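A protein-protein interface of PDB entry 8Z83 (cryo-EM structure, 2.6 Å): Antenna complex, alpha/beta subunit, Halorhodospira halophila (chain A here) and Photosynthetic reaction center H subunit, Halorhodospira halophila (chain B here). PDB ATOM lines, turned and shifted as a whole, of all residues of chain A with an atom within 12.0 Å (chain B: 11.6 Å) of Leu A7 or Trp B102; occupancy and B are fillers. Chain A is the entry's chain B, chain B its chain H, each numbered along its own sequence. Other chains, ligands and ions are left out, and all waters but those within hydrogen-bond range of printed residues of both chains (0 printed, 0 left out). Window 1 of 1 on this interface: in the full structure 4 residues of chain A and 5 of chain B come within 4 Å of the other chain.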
ATOM      1  N   SER A   6       2.630  15.170  -2.322  1.00  0.00           N
ATOM      2  CA  SER A   6       3.761  14.833  -3.175  1.00  0.00           C
ATOM      3  C   SER A   6       3.871  15.824  -4.321  1.00  0.00           C
ATOM      4  O   SER A   6       2.897  16.064  -5.029  1.00  0.00           O
ATOM      5  CB  SER A   6       3.623  13.413  -3.723  1.00  0.00           C
ATOM      6  OG  SER A   6       2.520  13.304  -4.603  1.00  0.00           O
ATOM      7  N   LEU A   7       5.051  16.406  -4.515  1.00  0.00           N
ATOM      8  CA  LEU A   7       5.220  17.365  -5.603  1.00  0.00           C
ATOM      9  C   LEU A   7       5.543  16.700  -6.933  1.00  0.00           C
ATOM     10  O   LEU A   7       6.438  17.141  -7.654  1.00  0.00           O
ATOM     11  CB  LEU A   7       6.305  18.371  -5.229  1.00  0.00           C
ATOM     12  CG  LEU A   7       7.346  17.926  -4.201  1.00  0.00           C
ATOM     13  CD1 LEU A   7       8.740  18.370  -4.600  1.00  0.00           C
ATOM     14  CD2 LEU A   7       6.991  18.497  -2.850  1.00  0.00           C
ATOM     15  N   THR A   8       4.794  15.661  -7.289  1.00  0.00           N
ATOM     16  CA  THR A   8       4.835  15.053  -8.613  1.00  0.00           C
ATOM     17  C   THR A   8       3.458  14.721  -9.146  1.00  0.00           C
ATOM     18  O   THR A   8       3.327  14.472 -10.351  1.00  0.00           O
ATOM     19  CB  THR A   8       5.674  13.762  -8.608  1.00  0.00           C
ATOM     20  OG1 THR A   8       5.147  12.837  -7.649  1.00  0.00           O
ATOM     21  CG2 THR A   8       7.119  14.058  -8.277  1.00  0.00           C
ATOM     22  N   GLY A   9       2.434  14.704  -8.296  1.00  0.00           N
ATOM     23  CA  GLY A   9       1.114  14.273  -8.668  1.00  0.00           C
ATOM     24  C   GLY A   9       0.848  12.806  -8.433  1.00  0.00           C
ATOM     25  O   GLY A   9      -0.317  12.410  -8.325  1.00  0.00           O
ATOM     26  N   LEU A  10       1.893  11.990  -8.341  1.00  0.00           N
ATOM     27  CA  LEU A  10       1.706  10.562  -8.146  1.00  0.00           C
ATOM     28  C   LEU A  10       1.236  10.280  -6.728  1.00  0.00           C
ATOM     29  O   LEU A  10       1.798  10.800  -5.760  1.00  0.00           O
ATOM     30  CB  LEU A  10       3.004   9.809  -8.434  1.00  0.00           C
ATOM     31  CG  LEU A  10       3.147   9.237  -9.844  1.00  0.00           C
ATOM     32  CD1 LEU A  10       3.162  10.348 -10.880  1.00  0.00           C
ATOM     33  CD2 LEU A  10       4.391   8.376  -9.953  1.00  0.00           C
ATOM     34  N   SER A  11       0.194   9.464  -6.610  1.00  0.00           N
ATOM     35  CA  SER A  11      -0.259   8.991  -5.317  1.00  0.00           C
ATOM     36  C   SER A  11       0.701   7.933  -4.784  1.00  0.00           C
ATOM     37  O   SER A  11       1.637   7.507  -5.464  1.00  0.00           O
ATOM     38  CB  SER A  11      -1.674   8.426  -5.418  1.00  0.00           C
ATOM     39  OG  SER A  11      -1.761   7.446  -6.439  1.00  0.00           O
ATOM     40  N   ASP A  12       0.452   7.506  -3.544  1.00  0.00           N
ATOM     41  CA  ASP A  12       1.291   6.477  -2.937  1.00  0.00           C
ATOM     42  C   ASP A  12       1.255   5.190  -3.747  1.00  0.00           C
ATOM     43  O   ASP A  12       2.299   4.578  -3.998  1.00  0.00           O
ATOM     44  CB  ASP A  12       0.843   6.211  -1.498  1.00  0.00           C
ATOM     45  CG  ASP A  12       0.867   7.456  -0.642  1.00  0.00           C
ATOM     46  OD1 ASP A  12       0.006   8.333  -0.852  1.00  0.00           O
ATOM     47  OD2 ASP A  12       1.744   7.558   0.243  1.00  0.00           O
ATOM     48  N   GLU A  14       0.471   4.777  -6.953  1.00  0.00           N
ATOM     49  CA  GLU A  14       1.134   4.953  -8.241  1.00  0.00           C
ATOM     50  C   GLU A  14       2.642   5.088  -8.084  1.00  0.00           C
ATOM     51  O   GLU A  14       3.395   4.647  -8.961  1.00  0.00           O
ATOM     52  CB  GLU A  14       0.560   6.166  -8.966  1.00  0.00           C
ATOM     53  CG  GLU A  14      -0.842   5.938  -9.494  1.00  0.00           C
ATOM     54  CD  GLU A  14      -1.548   7.227  -9.860  1.00  0.00           C
ATOM     55  OE1 GLU A  14      -1.206   8.277  -9.277  1.00  0.00           O
ATOM     56  OE2 GLU A  14      -2.442   7.189 -10.728  1.00  0.00           O
ATOM     57  N   ALA A  15       3.101   5.699  -6.990  1.00  0.00           N
ATOM     58  CA  ALA A  15       4.531   5.725  -6.706  1.00  0.00           C
ATOM     59  C   ALA A  15       5.069   4.319  -6.486  1.00  0.00           C
ATOM     60  O   ALA A  15       6.174   3.990  -6.933  1.00  0.00           O
ATOM     61  CB  ALA A  15       4.809   6.603  -5.487  1.00  0.00           C
ATOM     62  N   PHE A  18       5.072   2.518  -9.989  1.00  0.00           N
ATOM     63  CA  PHE A  18       6.225   2.908 -10.792  1.00  0.00           C
ATOM     64  C   PHE A  18       7.504   2.299 -10.238  1.00  0.00           C
ATOM     65  O   PHE A  18       8.372   1.863 -11.000  1.00  0.00           O
ATOM     66  CB  PHE A  18       6.343   4.431 -10.858  1.00  0.00           C
ATOM     67  CG  PHE A  18       7.563   4.913 -11.590  1.00  0.00           C
ATOM     68  CD1 PHE A  18       7.580   4.974 -12.970  1.00  0.00           C
ATOM     69  CD2 PHE A  18       8.696   5.295 -10.899  1.00  0.00           C
ATOM     70  CE1 PHE A  18       8.703   5.406 -13.645  1.00  0.00           C
ATOM     71  CE2 PHE A  18       9.818   5.730 -11.570  1.00  0.00           C
ATOM     72  CZ  PHE A  18       9.820   5.788 -12.943  1.00  0.00           C
ATOM     73  N   ALA B  45      10.070  30.859  -5.521  1.00  0.00           N
ATOM     74  CA  ALA B  45      10.172  29.402  -5.507  1.00  0.00           C
ATOM     75  C   ALA B  45       8.821  28.851  -5.070  1.00  0.00           C
ATOM     76  O   ALA B  45       8.513  28.810  -3.878  1.00  0.00           O
ATOM     77  CB  ALA B  45      11.297  28.945  -4.587  1.00  0.00           C
ATOM     78  N   GLU B  46       8.019  28.423  -6.040  1.00  0.00           N
ATOM     79  CA  GLU B  46       6.653  28.009  -5.762  1.00  0.00           C
ATOM     80  C   GLU B  46       6.625  26.727  -4.934  1.00  0.00           C
ATOM     81  O   GLU B  46       7.624  26.019  -4.795  1.00  0.00           O
ATOM     82  CB  GLU B  46       5.878  27.824  -7.066  1.00  0.00           C
ATOM     83  CG  GLU B  46       6.035  28.989  -8.028  1.00  0.00           C
ATOM     84  CD  GLU B  46       4.903  29.082  -9.031  1.00  0.00           C
ATOM     85  OE1 GLU B  46       3.874  28.403  -8.832  1.00  0.00           O
ATOM     86  OE2 GLU B  46       5.040  29.838 -10.015  1.00  0.00           O
ATOM     87  N   ALA B  47       5.445  26.440  -4.378  1.00  0.00           N
ATOM     88  CA  ALA B  47       5.312  25.383  -3.379  1.00  0.00           C
ATOM     89  C   ALA B  47       5.750  24.027  -3.917  1.00  0.00           C
ATOM     90  O   ALA B  47       6.389  23.248  -3.202  1.00  0.00           O
ATOM     91  CB  ALA B  47       3.869  25.321  -2.881  1.00  0.00           C
ATOM     92  N   ASN B  48       5.418  23.723  -5.173  1.00  0.00           N
ATOM     93  CA  ASN B  48       5.775  22.428  -5.741  1.00  0.00           C
ATOM     94  C   ASN B  48       7.274  22.268  -5.962  1.00  0.00           C
ATOM     95  O   ASN B  48       7.724  21.151  -6.237  1.00  0.00           O
ATOM     96  CB  ASN B  48       5.028  22.209  -7.059  1.00  0.00           C
ATOM     97  CG  ASN B  48       5.363  23.256  -8.106  1.00  0.00           C
ATOM     98  OD1 ASN B  48       5.829  24.349  -7.789  1.00  0.00           O
ATOM     99  ND2 ASN B  48       5.117  22.923  -9.367  1.00  0.00           N
ATOM    100  N   GLU B  49       8.054  23.340  -5.850  1.00  0.00           N
ATOM    101  CA  GLU B  49       9.490  23.267  -6.077  1.00  0.00           C
ATOM    102  C   GLU B  49      10.277  22.842  -4.841  1.00  0.00           C
ATOM    103  O   GLU B  49      11.458  22.504  -4.966  1.00  0.00           O
ATOM    104  CB  GLU B  49      10.002  24.623  -6.577  1.00  0.00           C
ATOM    105  CG  GLU B  49      11.326  24.569  -7.323  1.00  0.00           C
ATOM    106  CD  GLU B  49      12.435  25.316  -6.606  1.00  0.00           C
ATOM    107  OE1 GLU B  49      12.138  26.015  -5.617  1.00  0.00           O
ATOM    108  OE2 GLU B  49      13.604  25.204  -7.031  1.00  0.00           O
ATOM    109  N   ASN B  50       9.658  22.834  -3.662  1.00  0.00           N
ATOM    110  CA  ASN B  50      10.355  22.565  -2.414  1.00  0.00           C
ATOM    111  C   ASN B  50       9.692  21.417  -1.666  1.00  0.00           C
ATOM    112  O   ASN B  50       8.488  21.180  -1.796  1.00  0.00           O
ATOM    113  CB  ASN B  50      10.386  23.806  -1.513  1.00  0.00           C
ATOM    114  CG  ASN B  50      11.085  24.983  -2.161  1.00  0.00           C
ATOM    115  OD1 ASN B  50      11.965  24.811  -3.001  1.00  0.00           O
ATOM    116  ND2 ASN B  50      10.694  26.190  -1.771  1.00  0.00           N
ATOM    117  N   CYS B  51      10.497  20.706  -0.872  1.00  0.00           N
ATOM    118  CA  CYS B  51       9.969  19.658  -0.009  1.00  0.00           C
ATOM    119  C   CYS B  51       9.163  20.219   1.153  1.00  0.00           C
ATOM    120  O   CYS B  51       8.349  19.492   1.733  1.00  0.00           O
ATOM    121  CB  CYS B  51      11.107  18.796   0.538  1.00  0.00           C
ATOM    122  SG  CYS B  51      12.245  18.153  -0.700  1.00  0.00           S
ATOM    123  N   ASN B  52       9.375  21.488   1.513  1.00  0.00           N
ATOM    124  CA  ASN B  52       8.617  22.120   2.584  1.00  0.00           C
ATOM    125  C   ASN B  52       7.246  22.603   2.132  1.00  0.00           C
ATOM    126  O   ASN B  52       6.447  23.022   2.978  1.00  0.00           O
ATOM    127  CB  ASN B  52       9.412  23.290   3.177  1.00  0.00           C
ATOM    128  CG  ASN B  52      10.109  24.123   2.120  1.00  0.00           C
ATOM    129  OD1 ASN B  52       9.477  24.898   1.405  1.00  0.00           O
ATOM    130  ND2 ASN B  52      11.425  23.970   2.022  1.00  0.00           N
ATOM    131  N   ARG B  53       6.966  22.561   0.828  1.00  0.00           N
ATOM    132  CA  ARG B  53       5.648  22.869   0.270  1.00  0.00           C
ATOM    133  C   ARG B  53       5.193  24.289   0.597  1.00  0.00           C
ATOM    134  O   ARG B  53       3.996  24.547   0.738  1.00  0.00           O
ATOM    135  CB  ARG B  53       4.598  21.859   0.740  1.00  0.00           C
ATOM    136  CG  ARG B  53       5.004  20.411   0.556  1.00  0.00           C
ATOM    137  CD  ARG B  53       3.877  19.474   0.952  1.00  0.00           C
ATOM    138  NE  ARG B  53       4.277  18.075   0.872  1.00  0.00           N
ATOM    139  CZ  ARG B  53       4.306  17.367  -0.248  1.00  0.00           C
ATOM    140  NH1 ARG B  53       3.979  17.903  -1.412  1.00  0.00           N
ATOM    141  NH2 ARG B  53       4.675  16.091  -0.200  1.00  0.00           N
ATOM    142  N   THR B  54       6.132  25.226   0.717  1.00  0.00           N
ATOM    143  CA  THR B  54       5.765  26.616   0.943  1.00  0.00           C
ATOM    144  C   THR B  54       6.570  27.512   0.011  1.00  0.00           C
ATOM    145  O   THR B  54       7.757  27.249  -0.235  1.00  0.00           O
ATOM    146  CB  THR B  54       5.982  27.048   2.403  1.00  0.00           C
ATOM    147  OG1 THR B  54       5.718  28.450   2.536  1.00  0.00           O
ATOM    148  CG2 THR B  54       7.398  26.757   2.857  1.00  0.00           C
ATOM    149  N   PRO B  55       5.948  28.550  -0.542  1.00  0.00           N
ATOM    150  CA  PRO B  55       6.683  29.464  -1.420  1.00  0.00           C
ATOM    151  C   PRO B  55       7.827  30.143  -0.684  1.00  0.00           C
ATOM    152  O   PRO B  55       7.701  30.531   0.479  1.00  0.00           O
ATOM    153  CB  PRO B  55       5.611  30.467  -1.858  1.00  0.00           C
ATOM    154  CG  PRO B  55       4.332  29.713  -1.733  1.00  0.00           C
ATOM    155  CD  PRO B  55       4.507  28.847  -0.522  1.00  0.00           C
ATOM    156  N   GLU B  56       8.952  30.285  -1.379  1.00  0.00           N
ATOM    157  CA  GLU B  56      10.155  30.865  -0.805  1.00  0.00           C
ATOM    158  C   GLU B  56      10.777  31.834  -1.797  1.00  0.00           C
ATOM    159  O   GLU B  56      10.553  31.751  -3.006  1.00  0.00           O
ATOM    160  CB  GLU B  56      11.181  29.791  -0.421  1.00  0.00           C
ATOM    161  CG  GLU B  56      10.909  29.113   0.905  1.00  0.00           C
ATOM    162  CD  GLU B  56      11.927  28.033   1.224  1.00  0.00           C
ATOM    163  OE1 GLU B  56      12.858  27.833   0.414  1.00  0.00           O
ATOM    164  OE2 GLU B  56      11.794  27.385   2.283  1.00  0.00           O
ATOM    165  N   LYS B  58      14.307  33.075  -3.362  1.00  0.00           N
ATOM    166  CA  LYS B  58      15.681  32.647  -3.587  1.00  0.00           C
ATOM    167  C   LYS B  58      16.492  33.820  -4.111  1.00  0.00           C
ATOM    168  O   LYS B  58      16.072  34.501  -5.052  1.00  0.00           O
ATOM    169  CB  LYS B  58      15.748  31.481  -4.574  1.00  0.00           C
ATOM    170  CG  LYS B  58      15.637  30.109  -3.935  1.00  0.00           C
ATOM    171  CD  LYS B  58      16.032  29.024  -4.922  1.00  0.00           C
ATOM    172  CE  LYS B  58      16.073  27.655  -4.268  1.00  0.00           C
ATOM    173  NZ  LYS B  58      16.652  26.627  -5.176  1.00  0.00           N
ATOM    174  N   GLU B  97      -3.304  26.314 -16.439  1.00  0.00           N
ATOM    175  CA  GLU B  97      -3.115  25.215 -15.511  1.00  0.00           C
ATOM    176  C   GLU B  97      -1.867  24.449 -15.932  1.00  0.00           C
ATOM    177  O   GLU B  97      -1.734  24.087 -17.113  1.00  0.00           O
ATOM    178  CB  GLU B  97      -4.342  24.296 -15.496  1.00  0.00           C
ATOM    179  CG  GLU B  97      -4.849  23.950 -14.105  1.00  0.00           C
ATOM    180  CD  GLU B  97      -4.285  22.643 -13.584  1.00  0.00           C
ATOM    181  OE1 GLU B  97      -3.861  21.806 -14.408  1.00  0.00           O
ATOM    182  OE2 GLU B  97      -4.266  22.453 -12.350  1.00  0.00           O
ATOM    183  N   PRO B  98      -0.930  24.201 -15.020  1.00  0.00           N
ATOM    184  CA  PRO B  98       0.255  23.418 -15.386  1.00  0.00           C
ATOM    185  C   PRO B  98      -0.140  22.028 -15.861  1.00  0.00           C
ATOM    186  O   PRO B  98      -1.063  21.408 -15.328  1.00  0.00           O
ATOM    187  CB  PRO B  98       1.063  23.367 -14.084  1.00  0.00           C
ATOM    188  CG  PRO B  98       0.067  23.643 -13.003  1.00  0.00           C
ATOM    189  CD  PRO B  98      -0.926  24.587 -13.599  1.00  0.00           C
ATOM    190  N   THR B  99       0.562  21.549 -16.891  1.00  0.00           N
ATOM    191  CA  THR B  99       0.241  20.241 -17.453  1.00  0.00           C
ATOM    192  C   THR B  99       0.518  19.124 -16.460  1.00  0.00           C
ATOM    193  O   THR B  99      -0.163  18.091 -16.483  1.00  0.00           O
ATOM    194  CB  THR B  99       1.026  20.009 -18.744  1.00  0.00           C
ATOM    195  OG1 THR B  99       2.426  19.936 -18.450  1.00  0.00           O
ATOM    196  CG2 THR B  99       0.781  21.140 -19.728  1.00  0.00           C
ATOM    197  N   ALA B 100       1.502  19.305 -15.587  1.00  0.00           N
ATOM    198  CA  ALA B 100       1.844  18.329 -14.568  1.00  0.00           C
ATOM    199  C   ALA B 100       2.112  19.049 -13.256  1.00  0.00           C
ATOM    200  O   ALA B 100       2.537  20.211 -13.259  1.00  0.00           O
ATOM    201  CB  ALA B 100       3.070  17.500 -14.976  1.00  0.00           C
ATOM    202  N   PRO B 101       1.863  18.393 -12.119  1.00  0.00           N
ATOM    203  CA  PRO B 101       1.986  19.091 -10.829  1.00  0.00           C
ATOM    204  C   PRO B 101       3.411  19.437 -10.432  1.00  0.00           C
ATOM    205  O   PRO B 101       3.592  20.299  -9.565  1.00  0.00           O
ATOM    206  CB  PRO B 101       1.359  18.103  -9.836  1.00  0.00           C
ATOM    207  CG  PRO B 101       0.516  17.204 -10.670  1.00  0.00           C
ATOM    208  CD  PRO B 101       1.244  17.068 -11.963  1.00  0.00           C
ATOM    209  N   TRP B 102       4.423  18.808 -11.020  1.00  0.00           N
ATOM    210  CA  TRP B 102       5.782  19.052 -10.566  1.00  0.00           C
ATOM    211  C   TRP B 102       6.333  20.351 -11.148  1.00  0.00           C
ATOM    212  O   TRP B 102       5.841  20.879 -12.148  1.00  0.00           O
ATOM    213  CB  TRP B 102       6.695  17.881 -10.926  1.00  0.00           C
ATOM    214  CG  TRP B 102       6.405  17.255 -12.246  1.00  0.00           C
ATOM    215  CD1 TRP B 102       5.566  16.211 -12.485  1.00  0.00           C
ATOM    216  CD2 TRP B 102       6.962  17.621 -13.515  1.00  0.00           C
ATOM    217  NE1 TRP B 102       5.562  15.904 -13.820  1.00  0.00           N
ATOM    218  CE2 TRP B 102       6.411  16.756 -14.475  1.00  0.00           C
ATOM    219  CE3 TRP B 102       7.872  18.596 -13.930  1.00  0.00           C
ATOM    220  CZ2 TRP B 102       6.737  16.835 -15.825  1.00  0.00           C
ATOM    221  CZ3 TRP B 102       8.194  18.674 -15.272  1.00  0.00           C
ATOM    222  CH2 TRP B 102       7.629  17.800 -16.202  1.00  0.00           C
ATOM    223  N   ASP B 103       7.366  20.872 -10.490  1.00  0.00           N
ATOM    224  CA  ASP B 103       7.964  22.132 -10.906  1.00  0.00           C
ATOM    225  C   ASP B 103       8.688  21.966 -12.233  1.00  0.00           C
ATOM    226  O   ASP B 103       9.334  20.945 -12.485  1.00  0.00           O
ATOM    227  CB  ASP B 103       8.929  22.647  -9.840  1.00  0.00           C
ATOM    228  CG  ASP B 103      10.121  21.731  -9.638  1.00  0.00           C
ATOM    229  OD1 ASP B 103       9.920  20.504  -9.511  1.00  0.00           O
ATOM    230  OD2 ASP B 103      11.261  22.242  -9.615  1.00  0.00           O
ATOM    231  N   GLY B 104       8.587  22.985 -13.081  1.00  0.00           N
ATOM    232  CA  GLY B 104       9.129  22.930 -14.416  1.00  0.00           C
ATOM    233  C   GLY B 104       8.156  22.478 -15.480  1.00  0.00           C
ATOM    234  O   GLY B 104       8.490  22.543 -16.669  1.00  0.00           O
ATOM    235  N   ALA B 105       6.970  22.017 -15.097  1.00  0.00           N
ATOM    236  CA  ALA B 105       5.975  21.641 -16.085  1.00  0.00           C
ATOM    237  C   ALA B 105       5.376  22.891 -16.728  1.00  0.00           C
ATOM    238  O   ALA B 105       5.094  23.870 -16.033  1.00  0.00           O
ATOM    239  CB  ALA B 105       4.873  20.799 -15.446  1.00  0.00           C
ATOM    240  N   PRO B 106       5.174  22.888 -18.041  1.00  0.00           N
ATOM    241  CA  PRO B 106       4.603  24.063 -18.703  1.00  0.00           C
ATOM    242  C   PRO B 106       3.139  24.256 -18.342  1.00  0.00           C
ATOM    243  O   PRO B 106       2.436  23.328 -17.939  1.00  0.00           O
ATOM    244  CB  PRO B 106       4.768  23.741 -20.189  1.00  0.00           C
ATOM    245  CG  PRO B 106       4.714  22.256 -20.238  1.00  0.00           C
ATOM    246  CD  PRO B 106       5.387  21.777 -18.980  1.00  0.00           C
ATOM    247  N   LEU B 107       2.686  25.497 -18.488  1.00  0.00           N
ATOM    248  CA  LEU B 107       1.301  25.856 -18.227  1.00  0.00           C
ATOM    249  C   LEU B 107       0.449  25.617 -19.464  1.00  0.00           C
ATOM    250  O   LEU B 107       0.864  25.912 -20.587  1.00  0.00           O
ATOM    251  CB  LEU B 107       1.192  27.321 -17.805  1.00  0.00           C
ATOM    252  CG  LEU B 107       1.798  27.719 -16.461  1.00  0.00           C
ATOM    253  CD1 LEU B 107       1.877  29.226 -16.357  1.00  0.00           C
ATOM    254  CD2 LEU B 107       0.976  27.151 -15.324  1.00  0.00           C
ATOM    255  N   GLU B 108      -0.746  25.080 -19.248  1.00  0.00           N
ATOM    256  CA  GLU B 108      -1.725  24.927 -20.316  1.00  0.00           C
ATOM    257  C   GLU B 108      -2.823  25.961 -20.125  1.00  0.00           C
ATOM    258  O   GLU B 108      -3.587  25.869 -19.152  1.00  0.00           O
ATOM    259  CB  GLU B 108      -2.315  23.517 -20.321  1.00  0.00           C
ATOM    260  CG  GLU B 108      -3.363  23.293 -21.399  1.00  0.00           C
ATOM    261  CD  GLU B 108      -2.785  23.350 -22.798  1.00  0.00           C
ATOM    262  OE1 GLU B 108      -1.583  23.058 -22.960  1.00  0.00           O
ATOM    263  OE2 GLU B 108      -3.533  23.690 -23.739  1.00  0.00           O
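The backbone NH of Ser A6 sits close to the guanidinium group of Arg B53 (3.1 Å).
The side-chain hydroxyl (OG) of Ser A6 is in hydrogen-bond range of the backbone carbonyl oxygen (O) of Leu A10 (2.9 Å).
The backbone carbonyl oxygen (O) of Thr B54 is in hydrogen-bond range of the side-chain amide nitrogen (ND2) of Asn B50 (3.5 Å).
OG1 of Thr A8 lies close to N of Leu A10 (3.4 Å).
The side-chain amide nitrogen (ND2) of Asn B50 lies within hydrogen-bond range of the side-chain carboxylate (OE1) of Glu B56, 3.5 Å away.
O of Pro B101 lies within hydrogen-bond range of ND2 of Asn B48, 3.0 Å away.
The side-chain amide nitrogen (ND2) of Asn B48 sits close to the backbone NH (N) of Asp B103 (3.2 Å).
Asn B48 touches Leu A7 (O to CB, 3.3 Å).
Leu A7 touches Asn B50 (CD2 to O, 3.2 Å).
Arg B53 touches Leu A7.
Leu A7 touches Trp B102 (O to CB, 3.4 Å).
Thr A8 touches Pro B101 (O to CD, 3.7 Å).
Thr A8 touches Trp B102.
CG of Pro B101 touches CA of Gly A9, 3.6 Å away.
Leu A7 touches just these residues of chain B: Asn B48 (3.3 Å), Asn B50 (3.2 Å), Arg B53 (3.4 Å) and Trp B102 (3.4 Å).
Trp B102 touches just these residues of chain A: Leu A7 (3.4 Å) and Thr A8 (3.5 Å).
Of chain B, only Pro B101 and Trp B102 come within 4 Å of Thr A8.
Asn B48 touches just one residue of chain A: Leu A7.
Of chain A, only Ser A6 and Leu A7 come within 4 Å of Arg B53.
Pro B101 touches just these residues of chain A: Thr A8 (3.7 Å) and Gly A9 (3.6 Å).
Asp B103 touches none of the printed residues of chain A.
No residue of chain A comes within 4 Å of Gly B104.
No residue of chain A comes within 4 Å of Ala B105.
Pro B106 touches none of the printed residues of chain A.
Of the printed residues of chain A, Asn B50 touches Leu A7 (3.2 Å).
The nearest residue of chain B that does not touch Leu A7 is Cys B51 (4.3 Å).
The nearest residue of chain A that does not touch Trp B102 is Gly A9 (5.3 Å).
The nearest printed residue of chain A that does not touch Asn B50 is Ser A6 (7.5 Å).
Of the 25 printed residues of chain B, 5 touch a printed residue of chain A.
Printed residues of chain A that touch a printed residue of chain B: Ser A6, Leu A7, Thr A8 and Gly A9.
Hydrophobic or aromatic side chains of chain A that line the printed part of chain B: Leu A7.
Among the printed residues, no Asp or Glu carboxylate lies within 4 Å of a Lys or Arg side-chain nitrogen of the other chain.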
